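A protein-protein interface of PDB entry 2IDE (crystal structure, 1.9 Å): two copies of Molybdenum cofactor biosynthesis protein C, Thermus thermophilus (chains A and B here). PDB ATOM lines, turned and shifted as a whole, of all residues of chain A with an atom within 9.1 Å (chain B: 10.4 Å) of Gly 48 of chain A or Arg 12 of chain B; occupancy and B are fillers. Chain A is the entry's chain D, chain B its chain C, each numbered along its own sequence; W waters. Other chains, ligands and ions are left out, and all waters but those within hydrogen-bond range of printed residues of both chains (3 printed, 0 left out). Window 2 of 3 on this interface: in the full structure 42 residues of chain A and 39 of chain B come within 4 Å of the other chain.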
ATOM      1  N   ALA A  41      14.705  24.296 -28.239  1.00  0.00           N
ATOM      2  CA  ALA A  41      15.586  23.144 -28.088  1.00  0.00           C
ATOM      3  C   ALA A  41      15.480  22.596 -26.667  1.00  0.00           C
ATOM      4  O   ALA A  41      15.376  21.386 -26.455  1.00  0.00           O
ATOM      5  CB  ALA A  41      17.026  23.547 -28.394  1.00  0.00           C
ATOM      6  N   LEU A  42      15.497  23.499 -25.693  1.00  0.00           N
ATOM      7  CA  LEU A  42      15.406  23.112 -24.292  1.00  0.00           C
ATOM      8  C   LEU A  42      14.142  22.297 -24.027  1.00  0.00           C
ATOM      9  O   LEU A  42      14.194  21.233 -23.413  1.00  0.00           O
ATOM     10  CB  LEU A  42      15.390  24.360 -23.398  1.00  0.00           C
ATOM     11  CG  LEU A  42      16.200  24.330 -22.099  1.00  0.00           C
ATOM     12  CD1 LEU A  42      15.706  25.442 -21.182  1.00  0.00           C
ATOM     13  CD2 LEU A  42      16.067  22.979 -21.419  1.00  0.00           C
ATOM     14  N   LYS A  44      12.523  20.569 -25.967  1.00  0.00           N
ATOM     15  CA  LYS A  44      12.548  19.312 -26.709  1.00  0.00           C
ATOM     16  C   LYS A  44      13.560  18.310 -26.147  1.00  0.00           C
ATOM     17  O   LYS A  44      13.706  17.206 -26.669  1.00  0.00           O
ATOM     18  CB  LYS A  44      12.838  19.591 -28.186  1.00  0.00           C
ATOM     19  CG  LYS A  44      11.630  20.137 -28.940  1.00  0.00           C
ATOM     20  CD  LYS A  44      12.028  21.086 -30.064  1.00  0.00           C
ATOM     21  CE  LYS A  44      12.911  20.417 -31.105  1.00  0.00           C
ATOM     22  NZ  LYS A  44      13.252  21.362 -32.208  1.00  0.00           N
ATOM     23  N   GLY A  45      14.251  18.700 -25.080  1.00  0.00           N
ATOM     24  CA  GLY A  45      15.221  17.813 -24.461  1.00  0.00           C
ATOM     25  C   GLY A  45      16.678  18.190 -24.659  1.00  0.00           C
ATOM     26  O   GLY A  45      17.570  17.516 -24.142  1.00  0.00           O
ATOM     27  N   GLY A  46      16.924  19.263 -25.406  1.00  0.00           N
ATOM     28  CA  GLY A  46      18.290  19.695 -25.647  1.00  0.00           C
ATOM     29  C   GLY A  46      18.653  19.714 -27.121  1.00  0.00           C
ATOM     30  O   GLY A  46      17.777  19.663 -27.987  1.00  0.00           O
ATOM     31  N   VAL A  47      19.950  19.783 -27.404  1.00  0.00           N
ATOM     32  CA  VAL A  47      20.440  19.816 -28.776  1.00  0.00           C
ATOM     33  C   VAL A  47      21.045  18.476 -29.172  1.00  0.00           C
ATOM     34  O   VAL A  47      21.693  18.363 -30.211  1.00  0.00           O
ATOM     35  CB  VAL A  47      21.513  20.909 -28.960  1.00  0.00           C
ATOM     36  CG1 VAL A  47      20.932  22.274 -28.609  1.00  0.00           C
ATOM     37  CG2 VAL A  47      22.726  20.601 -28.094  1.00  0.00           C
ATOM     38  N   GLY A  48      20.837  17.463 -28.335  1.00  0.00           N
ATOM     39  CA  GLY A  48      21.380  16.149 -28.627  1.00  0.00           C
ATOM     40  C   GLY A  48      22.515  15.750 -27.697  1.00  0.00           C
ATOM     41  O   GLY A  48      23.082  14.666 -27.840  1.00  0.00           O
ATOM     42  N   LYS A  49      22.849  16.626 -26.752  1.00  0.00           N
ATOM     43  CA  LYS A  49      23.917  16.363 -25.787  1.00  0.00           C
ATOM     44  C   LYS A  49      23.347  15.846 -24.473  1.00  0.00           C
ATOM     45  O   LYS A  49      24.085  15.339 -23.631  1.00  0.00           O
ATOM     46  CB  LYS A  49      24.723  17.637 -25.506  1.00  0.00           C
ATOM     47  CG  LYS A  49      25.667  18.043 -26.618  1.00  0.00           C
ATOM     48  CD  LYS A  49      26.398  19.342 -26.303  1.00  0.00           C
ATOM     49  CE  LYS A  49      27.328  19.207 -25.111  1.00  0.00           C
ATOM     50  NZ  LYS A  49      28.229  20.390 -25.016  1.00  0.00           N
ATOM     51  N   GLY A  50      22.034  15.987 -24.310  1.00  0.00           N
ATOM     52  CA  GLY A  50      21.368  15.544 -23.097  1.00  0.00           C
ATOM     53  C   GLY A  50      20.561  16.667 -22.464  1.00  0.00           C
ATOM     54  O   GLY A  50      20.572  17.792 -22.960  1.00  0.00           O
ATOM     55  N   ASP A  51      19.867  16.371 -21.367  1.00  0.00           N
ATOM     56  CA  ASP A  51      19.058  17.376 -20.676  1.00  0.00           C
ATOM     57  C   ASP A  51      19.934  18.486 -20.094  1.00  0.00           C
ATOM     58  O   ASP A  51      20.700  18.260 -19.158  1.00  0.00           O
ATOM     59  CB  ASP A  51      18.259  16.732 -19.546  1.00  0.00           C
ATOM     60  CG  ASP A  51      17.199  17.662 -18.981  1.00  0.00           C
ATOM     61  OD1 ASP A  51      17.537  18.803 -18.603  1.00  0.00           O
ATOM     62  OD2 ASP A  51      16.023  17.247 -18.914  1.00  0.00           O
ATOM     63  N   PRO A  52      19.815  19.710 -20.633  1.00  0.00           N
ATOM     64  CA  PRO A  52      20.597  20.863 -20.172  1.00  0.00           C
ATOM     65  C   PRO A  52      20.503  21.157 -18.675  1.00  0.00           C
ATOM     66  O   PRO A  52      21.512  21.425 -18.025  1.00  0.00           O
ATOM     67  CB  PRO A  52      20.037  22.016 -21.008  1.00  0.00           C
ATOM     68  CG  PRO A  52      19.635  21.330 -22.286  1.00  0.00           C
ATOM     69  CD  PRO A  52      18.950  20.086 -21.764  1.00  0.00           C
ATOM     70  N   VAL A  55      22.142  18.182 -16.388  1.00  0.00           N
ATOM     71  CA  VAL A  55      23.596  18.188 -16.381  1.00  0.00           C
ATOM     72  C   VAL A  55      24.156  19.423 -15.677  1.00  0.00           C
ATOM     73  O   VAL A  55      25.170  19.338 -14.982  1.00  0.00           O
ATOM     74  CB  VAL A  55      24.152  18.095 -17.816  1.00  0.00           C
ATOM     75  CG1 VAL A  55      25.669  18.105 -17.791  1.00  0.00           C
ATOM     76  CG2 VAL A  55      23.649  16.811 -18.474  1.00  0.00           C
ATOM     77  N   ASP A 126      26.859  25.428 -22.333  1.00  0.00           N
ATOM     78  CA  ASP A 126      27.496  24.345 -23.080  1.00  0.00           C
ATOM     79  C   ASP A 126      26.469  23.377 -23.663  1.00  0.00           C
ATOM     80  O   ASP A 126      26.668  22.831 -24.747  1.00  0.00           O
ATOM     81  CB  ASP A 126      28.453  23.562 -22.171  1.00  0.00           C
ATOM     82  CG  ASP A 126      29.112  22.384 -22.882  1.00  0.00           C
ATOM     83  OD1 ASP A 126      29.872  22.617 -23.847  1.00  0.00           O
ATOM     84  OD2 ASP A 126      28.867  21.224 -22.477  1.00  0.00           O
ATOM     85  N   MET A 127      25.372  23.175 -22.940  1.00  0.00           N
ATOM     86  CA  MET A 127      24.321  22.248 -23.364  1.00  0.00           C
ATOM     87  C   MET A 127      23.342  22.815 -24.397  1.00  0.00           C
ATOM     88  O   MET A 127      22.541  22.070 -24.963  1.00  0.00           O
ATOM     89  CB  MET A 127      23.526  21.772 -22.143  1.00  0.00           C
ATOM     90  CG  MET A 127      24.357  21.099 -21.057  1.00  0.00           C
ATOM     91  SD  MET A 127      25.161  19.588 -21.615  1.00  0.00           S
ATOM     92  CE  MET A 127      23.745  18.506 -21.746  1.00  0.00           C
ATOM     93  N   LEU A 128      23.395  24.123 -24.638  1.00  0.00           N
ATOM     94  CA  LEU A 128      22.486  24.750 -25.604  1.00  0.00           C
ATOM     95  C   LEU A 128      23.244  25.565 -26.655  1.00  0.00           C
ATOM     96  O   LEU A 128      22.659  26.089 -27.608  1.00  0.00           O
ATOM     97  CB  LEU A 128      21.476  25.636 -24.869  1.00  0.00           C
ATOM     98  CG  LEU A 128      20.437  24.891 -24.021  1.00  0.00           C
ATOM     99  CD1 LEU A 128      19.635  25.876 -23.189  1.00  0.00           C
ATOM    100  CD2 LEU A 128      19.514  24.090 -24.932  1.00  0.00           C
ATOM    101  N   ALA A 130      24.900  24.873 -29.176  1.00  0.00           N
ATOM    102  CA  ALA A 130      24.648  24.514 -30.568  1.00  0.00           C
ATOM    103  C   ALA A 130      23.433  25.215 -31.175  1.00  0.00           C
ATOM    104  O   ALA A 130      23.397  25.464 -32.377  1.00  0.00           O
ATOM    105  CB  ALA A 130      24.500  23.004 -30.695  1.00  0.00           C
ATOM    106  N   ALA A 131      22.437  25.524 -30.352  1.00  0.00           N
ATOM    107  CA  ALA A 131      21.242  26.207 -30.842  1.00  0.00           C
ATOM    108  C   ALA A 131      21.522  27.699 -31.019  1.00  0.00           C
ATOM    109  O   ALA A 131      21.115  28.306 -32.011  1.00  0.00           O
ATOM    110  CB  ALA A 131      20.085  26.007 -29.874  1.00  0.00           C
ATOM    111  N   GLY B   9      17.977  10.744 -25.123  1.00  0.00           N
ATOM    112  CA  GLY B   9      18.069  12.102 -24.515  1.00  0.00           C
ATOM    113  C   GLY B   9      19.044  12.139 -23.354  1.00  0.00           C
ATOM    114  O   GLY B   9      18.992  13.038 -22.514  1.00  0.00           O
ATOM    115  N   ARG B  10      19.942  11.163 -23.310  1.00  0.00           N
ATOM    116  CA  ARG B  10      20.919  11.090 -22.233  1.00  0.00           C
ATOM    117  C   ARG B  10      22.180  11.892 -22.541  1.00  0.00           C
ATOM    118  O   ARG B  10      22.462  12.203 -23.698  1.00  0.00           O
ATOM    119  CB  ARG B  10      21.286   9.629 -21.951  1.00  0.00           C
ATOM    120  CG  ARG B  10      22.187   8.969 -22.982  1.00  0.00           C
ATOM    121  CD  ARG B  10      22.509   7.541 -22.544  1.00  0.00           C
ATOM    122  NE  ARG B  10      23.631   6.958 -23.275  1.00  0.00           N
ATOM    123  CZ  ARG B  10      23.538   6.365 -24.460  1.00  0.00           C
ATOM    124  NH1 ARG B  10      22.364   6.262 -25.068  1.00  0.00           N
ATOM    125  NH2 ARG B  10      24.626   5.873 -25.040  1.00  0.00           N
ATOM    126  N   PRO B  11      22.949  12.248 -21.500  1.00  0.00           N
ATOM    127  CA  PRO B  11      24.189  13.018 -21.659  1.00  0.00           C
ATOM    128  C   PRO B  11      25.261  12.280 -22.458  1.00  0.00           C
ATOM    129  O   PRO B  11      25.413  11.065 -22.337  1.00  0.00           O
ATOM    130  CB  PRO B  11      24.641  13.252 -20.218  1.00  0.00           C
ATOM    131  CG  PRO B  11      23.356  13.236 -19.438  1.00  0.00           C
ATOM    132  CD  PRO B  11      22.599  12.098 -20.077  1.00  0.00           C
ATOM    133  N   ARG B  12      26.016  13.018 -23.263  1.00  0.00           N
ATOM    134  CA  ARG B  12      27.085  12.408 -24.044  1.00  0.00           C
ATOM    135  C   ARG B  12      28.119  13.419 -24.504  1.00  0.00           C
ATOM    136  O   ARG B  12      27.807  14.591 -24.722  1.00  0.00           O
ATOM    137  CB  ARG B  12      26.520  11.703 -25.282  1.00  0.00           C
ATOM    138  CG  ARG B  12      25.845  12.643 -26.285  1.00  0.00           C
ATOM    139  CD  ARG B  12      25.623  11.950 -27.619  1.00  0.00           C
ATOM    140  NE  ARG B  12      24.903  10.690 -27.461  1.00  0.00           N
ATOM    141  CZ  ARG B  12      23.633  10.592 -27.087  1.00  0.00           C
ATOM    142  NH1 ARG B  12      22.922  11.684 -26.833  1.00  0.00           N
ATOM    143  NH2 ARG B  12      23.074   9.395 -26.955  1.00  0.00           N
ATOM    144  N   MET B  13      29.361  12.970 -24.623  1.00  0.00           N
ATOM    145  CA  MET B  13      30.407  13.834 -25.129  1.00  0.00           C
ATOM    146  C   MET B  13      30.341  13.592 -26.629  1.00  0.00           C
ATOM    147  O   MET B  13      30.741  12.528 -27.122  1.00  0.00           O
ATOM    148  CB  MET B  13      31.771  13.441 -24.577  1.00  0.00           C
ATOM    149  CG  MET B  13      32.149  14.181 -23.309  1.00  0.00           C
ATOM    150  SD  MET B  13      33.857  13.880 -22.863  1.00  0.00           S
ATOM    151  CE  MET B  13      34.675  14.132 -24.471  1.00  0.00           C
ATOM    152  N   VAL B  14      29.793  14.576 -27.336  1.00  0.00           N
ATOM    153  CA  VAL B  14      29.614  14.520 -28.779  1.00  0.00           C
ATOM    154  C   VAL B  14      30.819  13.952 -29.512  1.00  0.00           C
ATOM    155  O   VAL B  14      31.950  14.380 -29.295  1.00  0.00           O
ATOM    156  CB  VAL B  14      29.296  15.920 -29.344  1.00  0.00           C
ATOM    157  CG1 VAL B  14      28.999  15.824 -30.834  1.00  0.00           C
ATOM    158  CG2 VAL B  14      28.109  16.521 -28.602  1.00  0.00           C
ATOM    159  N   ASP B  15      30.553  12.986 -30.385  1.00  0.00           N
ATOM    160  CA  ASP B  15      31.588  12.324 -31.171  1.00  0.00           C
ATOM    161  C   ASP B  15      32.102  13.250 -32.277  1.00  0.00           C
ATOM    162  O   ASP B  15      31.364  13.584 -33.207  1.00  0.00           O
ATOM    163  CB  ASP B  15      31.018  11.040 -31.784  1.00  0.00           C
ATOM    164  CG  ASP B  15      32.062  10.228 -32.529  1.00  0.00           C
ATOM    165  OD1 ASP B  15      31.669   9.281 -33.245  1.00  0.00           O
ATOM    166  OD2 ASP B  15      33.271  10.524 -32.399  1.00  0.00           O
ATOM    167  N   VAL B  16      33.361  13.664 -32.163  1.00  0.00           N
ATOM    168  CA  VAL B  16      33.993  14.548 -33.146  1.00  0.00           C
ATOM    169  C   VAL B  16      35.209  13.858 -33.761  1.00  0.00           C
ATOM    170  O   VAL B  16      36.062  14.494 -34.375  1.00  0.00           O
ATOM    171  CB  VAL B  16      34.457  15.872 -32.493  1.00  0.00           C
ATOM    172  CG1 VAL B  16      33.255  16.649 -31.978  1.00  0.00           C
ATOM    173  CG2 VAL B  16      35.421  15.585 -31.357  1.00  0.00           C
ATOM    174  N   ILE B  71      33.099  21.603 -16.804  1.00  0.00           N
ATOM    175  CA  ILE B  71      31.965  21.395 -17.704  1.00  0.00           C
ATOM    176  C   ILE B  71      31.957  19.904 -18.066  1.00  0.00           C
ATOM    177  O   ILE B  71      32.771  19.440 -18.867  1.00  0.00           O
ATOM    178  CB  ILE B  71      32.124  22.263 -18.977  1.00  0.00           C
ATOM    179  CG1 ILE B  71      32.472  23.702 -18.581  1.00  0.00           C
ATOM    180  CG2 ILE B  71      30.836  22.239 -19.798  1.00  0.00           C
ATOM    181  CD1 ILE B  71      31.486  24.351 -17.611  1.00  0.00           C
ATOM    182  N   PRO B  72      31.013  19.141 -17.486  1.00  0.00           N
ATOM    183  CA  PRO B  72      30.865  17.695 -17.693  1.00  0.00           C
ATOM    184  C   PRO B  72      31.097  17.112 -19.081  1.00  0.00           C
ATOM    185  O   PRO B  72      31.882  16.174 -19.235  1.00  0.00           O
ATOM    186  CB  PRO B  72      29.451  17.418 -17.182  1.00  0.00           C
ATOM    187  CG  PRO B  72      29.299  18.426 -16.083  1.00  0.00           C
ATOM    188  CD  PRO B  72      29.858  19.674 -16.739  1.00  0.00           C
ATOM    189  N   LEU B  73      30.425  17.655 -20.089  1.00  0.00           N
ATOM    190  CA  LEU B  73      30.556  17.119 -21.440  1.00  0.00           C
ATOM    191  C   LEU B  73      31.593  17.810 -22.320  1.00  0.00           C
ATOM    192  O   LEU B  73      31.663  17.563 -23.525  1.00  0.00           O
ATOM    193  CB  LEU B  73      29.187  17.141 -22.121  1.00  0.00           C
ATOM    194  CG  LEU B  73      28.084  16.476 -21.289  1.00  0.00           C
ATOM    195  CD1 LEU B  73      26.770  16.512 -22.053  1.00  0.00           C
ATOM    196  CD2 LEU B  73      28.482  15.033 -20.962  1.00  0.00           C
ATOM    197  N   CYS B  74      32.411  18.663 -21.715  1.00  0.00           N
ATOM    198  CA  CYS B  74      33.440  19.377 -22.459  1.00  0.00           C
ATOM    199  C   CYS B  74      34.581  18.427 -22.827  1.00  0.00           C
ATOM    200  O   CYS B  74      34.944  17.548 -22.040  1.00  0.00           O
ATOM    201  CB  CYS B  74      33.964  20.536 -21.609  1.00  0.00           C
ATOM    202  SG  CYS B  74      35.100  21.639 -22.439  1.00  0.00           S
ATOM    203  N   HIS B  75      35.132  18.596 -24.027  1.00  0.00           N
ATOM    204  CA  HIS B  75      36.238  17.755 -24.491  1.00  0.00           C
ATOM    205  C   HIS B  75      37.582  18.219 -23.936  1.00  0.00           C
ATOM    206  O   HIS B  75      37.863  19.414 -23.885  1.00  0.00           O
ATOM    207  CB  HIS B  75      36.366  17.786 -26.022  1.00  0.00           C
ATOM    208  CG  HIS B  75      35.200  17.202 -26.758  1.00  0.00           C
ATOM    209  ND1 HIS B  75      34.021  17.889 -26.950  1.00  0.00           N
ATOM    210  CD2 HIS B  75      35.042  16.005 -27.369  1.00  0.00           C
ATOM    211  CE1 HIS B  75      33.187  17.140 -27.649  1.00  0.00           C
ATOM    212  NE2 HIS B  75      33.781  15.991 -27.917  1.00  0.00           N
ATOM    213  N   THR B 107      37.195  20.430 -32.079  1.00  0.00           N
ATOM    214  CA  THR B 107      36.044  21.124 -31.499  1.00  0.00           C
ATOM    215  C   THR B 107      36.453  22.491 -30.950  1.00  0.00           C
ATOM    216  O   THR B 107      37.612  22.702 -30.604  1.00  0.00           O
ATOM    217  CB  THR B 107      35.395  20.288 -30.371  1.00  0.00           C
ATOM    218  OG1 THR B 107      35.273  18.925 -30.795  1.00  0.00           O
ATOM    219  CG2 THR B 107      34.000  20.815 -30.054  1.00  0.00           C
HETATM  220  O   HOH W   1      17.186  14.999 -22.712  1.00  0.00           O
HETATM  221  O   HOH W   2      28.337  19.923 -20.181  1.00  0.00           O
HETATM  222  O   HOH W   3      19.754  13.872 -20.210  1.00  0.00           O
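The guanidinium group (NH1) of Arg 12 of chain B sits at hydrogen-bond distance from the backbone carbonyl oxygen (O) of Arg 10 of chain B (3.2 Å).
O of Val 14 of chain B lies within hydrogen-bond range of NE2 of His 75 of chain B, at 2.8 Å.
NZ of Lys 49 of chain A is in salt-bridge range of OD2 of Asp 126 of chain A, at 2.7 Å.
Pro 11 of chain B touches Lys 49 of chain A (CA to O, 3.0 Å).
CG of Lys 49 of chain A touches CG2 of Val 14 of chain B, at 3.5 Å.
Lys 49 of chain A touches Leu 73 of chain B.
O of Gly 9 of chain B touches CA of Gly 50 of chain A, at 3.5 Å.
CA of Gly 50 of chain A touches O of Arg 10 of chain B, at 3.6 Å.
CA of Gly 50 of chain A touches N of Pro 11 of chain B (3.99 Å).
O of Gly 9 of chain B touches N of Asp 51 of chain A, 3.6 Å away.
Val 55 of chain A touches Pro 72 of chain B (CG1 to CB, 3.9 Å).
Asp 126 of chain A touches Ile 71 of chain B.
Leu 73 of chain B touches Met 127 of chain A (CD1 to SD, 3.5 Å).
Water W3 lies within hydrogen-bond range of O of Gly 9 of chain B (2.6 Å) and N of Asp 51 of chain A (2.8 Å).
Water W1 lies within hydrogen-bond range of the backbone carbonyl oxygen of Gly 9 of chain B (2.7 Å), the backbone carbonyl oxygen of Gly 45 of chain A (2.9 Å) and the backbone NH of Asp 51 of chain A (3.3 Å).
Water W2 lies within hydrogen-bond range of the side-chain carboxylate of Asp 126 of chain A, the backbone NH of Leu 73 of chain B and the side-chain sulfur of Met 127 of chain A.
Gly 45 of chain A touches none of the printed residues of chain B.
No residue of chain B comes within 4 Å of Val 47 of chain A.
Of the printed residues of chain A, Arg 10 of chain B touches Lys 49 (3.5 Å) and Gly 50 (3.6 Å).
Printed residues of chain A within 4 Å of Arg 12 of chain B: Gly 48 and Lys 49.
Val 16 of chain B touches none of the printed residues of chain A.
Of the printed residues of chain A, Pro 72 of chain B touches Val 55.
The nearest residue of chain B that does not touch Gly 48 of chain A is Arg 10 of chain B (4.9 Å).
The nearest residue of chain A that does not touch Arg 12 of chain B is Gly 50 of chain A (5.1 Å).
The nearest printed residue of chain A that does not touch Val 14 of chain B is Gly 48 of chain A (5.4 Å).
No position is printed for both chains.
The guanidinium group (NH1) of Arg 12 of chain B lies within hydrogen-bond range of the backbone carbonyl oxygen (O) of Gly 48 of chain A, at 3.2 Å.
The backbone NH (N) of Arg 12 of chain B sits at hydrogen-bond distance from the backbone carbonyl oxygen (O) of Lys 49 of chain A.
Hydrophobic or aromatic side chains of chain A that line the printed part of chain B: Val 55 and Met 127.
Along chain A the printed residues that touch a printed residue of chain B span positions 48 to 127.
Among the printed residues, no Asp or Glu carboxylate lies within 4 Å of a Lys or Arg side-chain nitrogen of the other chain.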
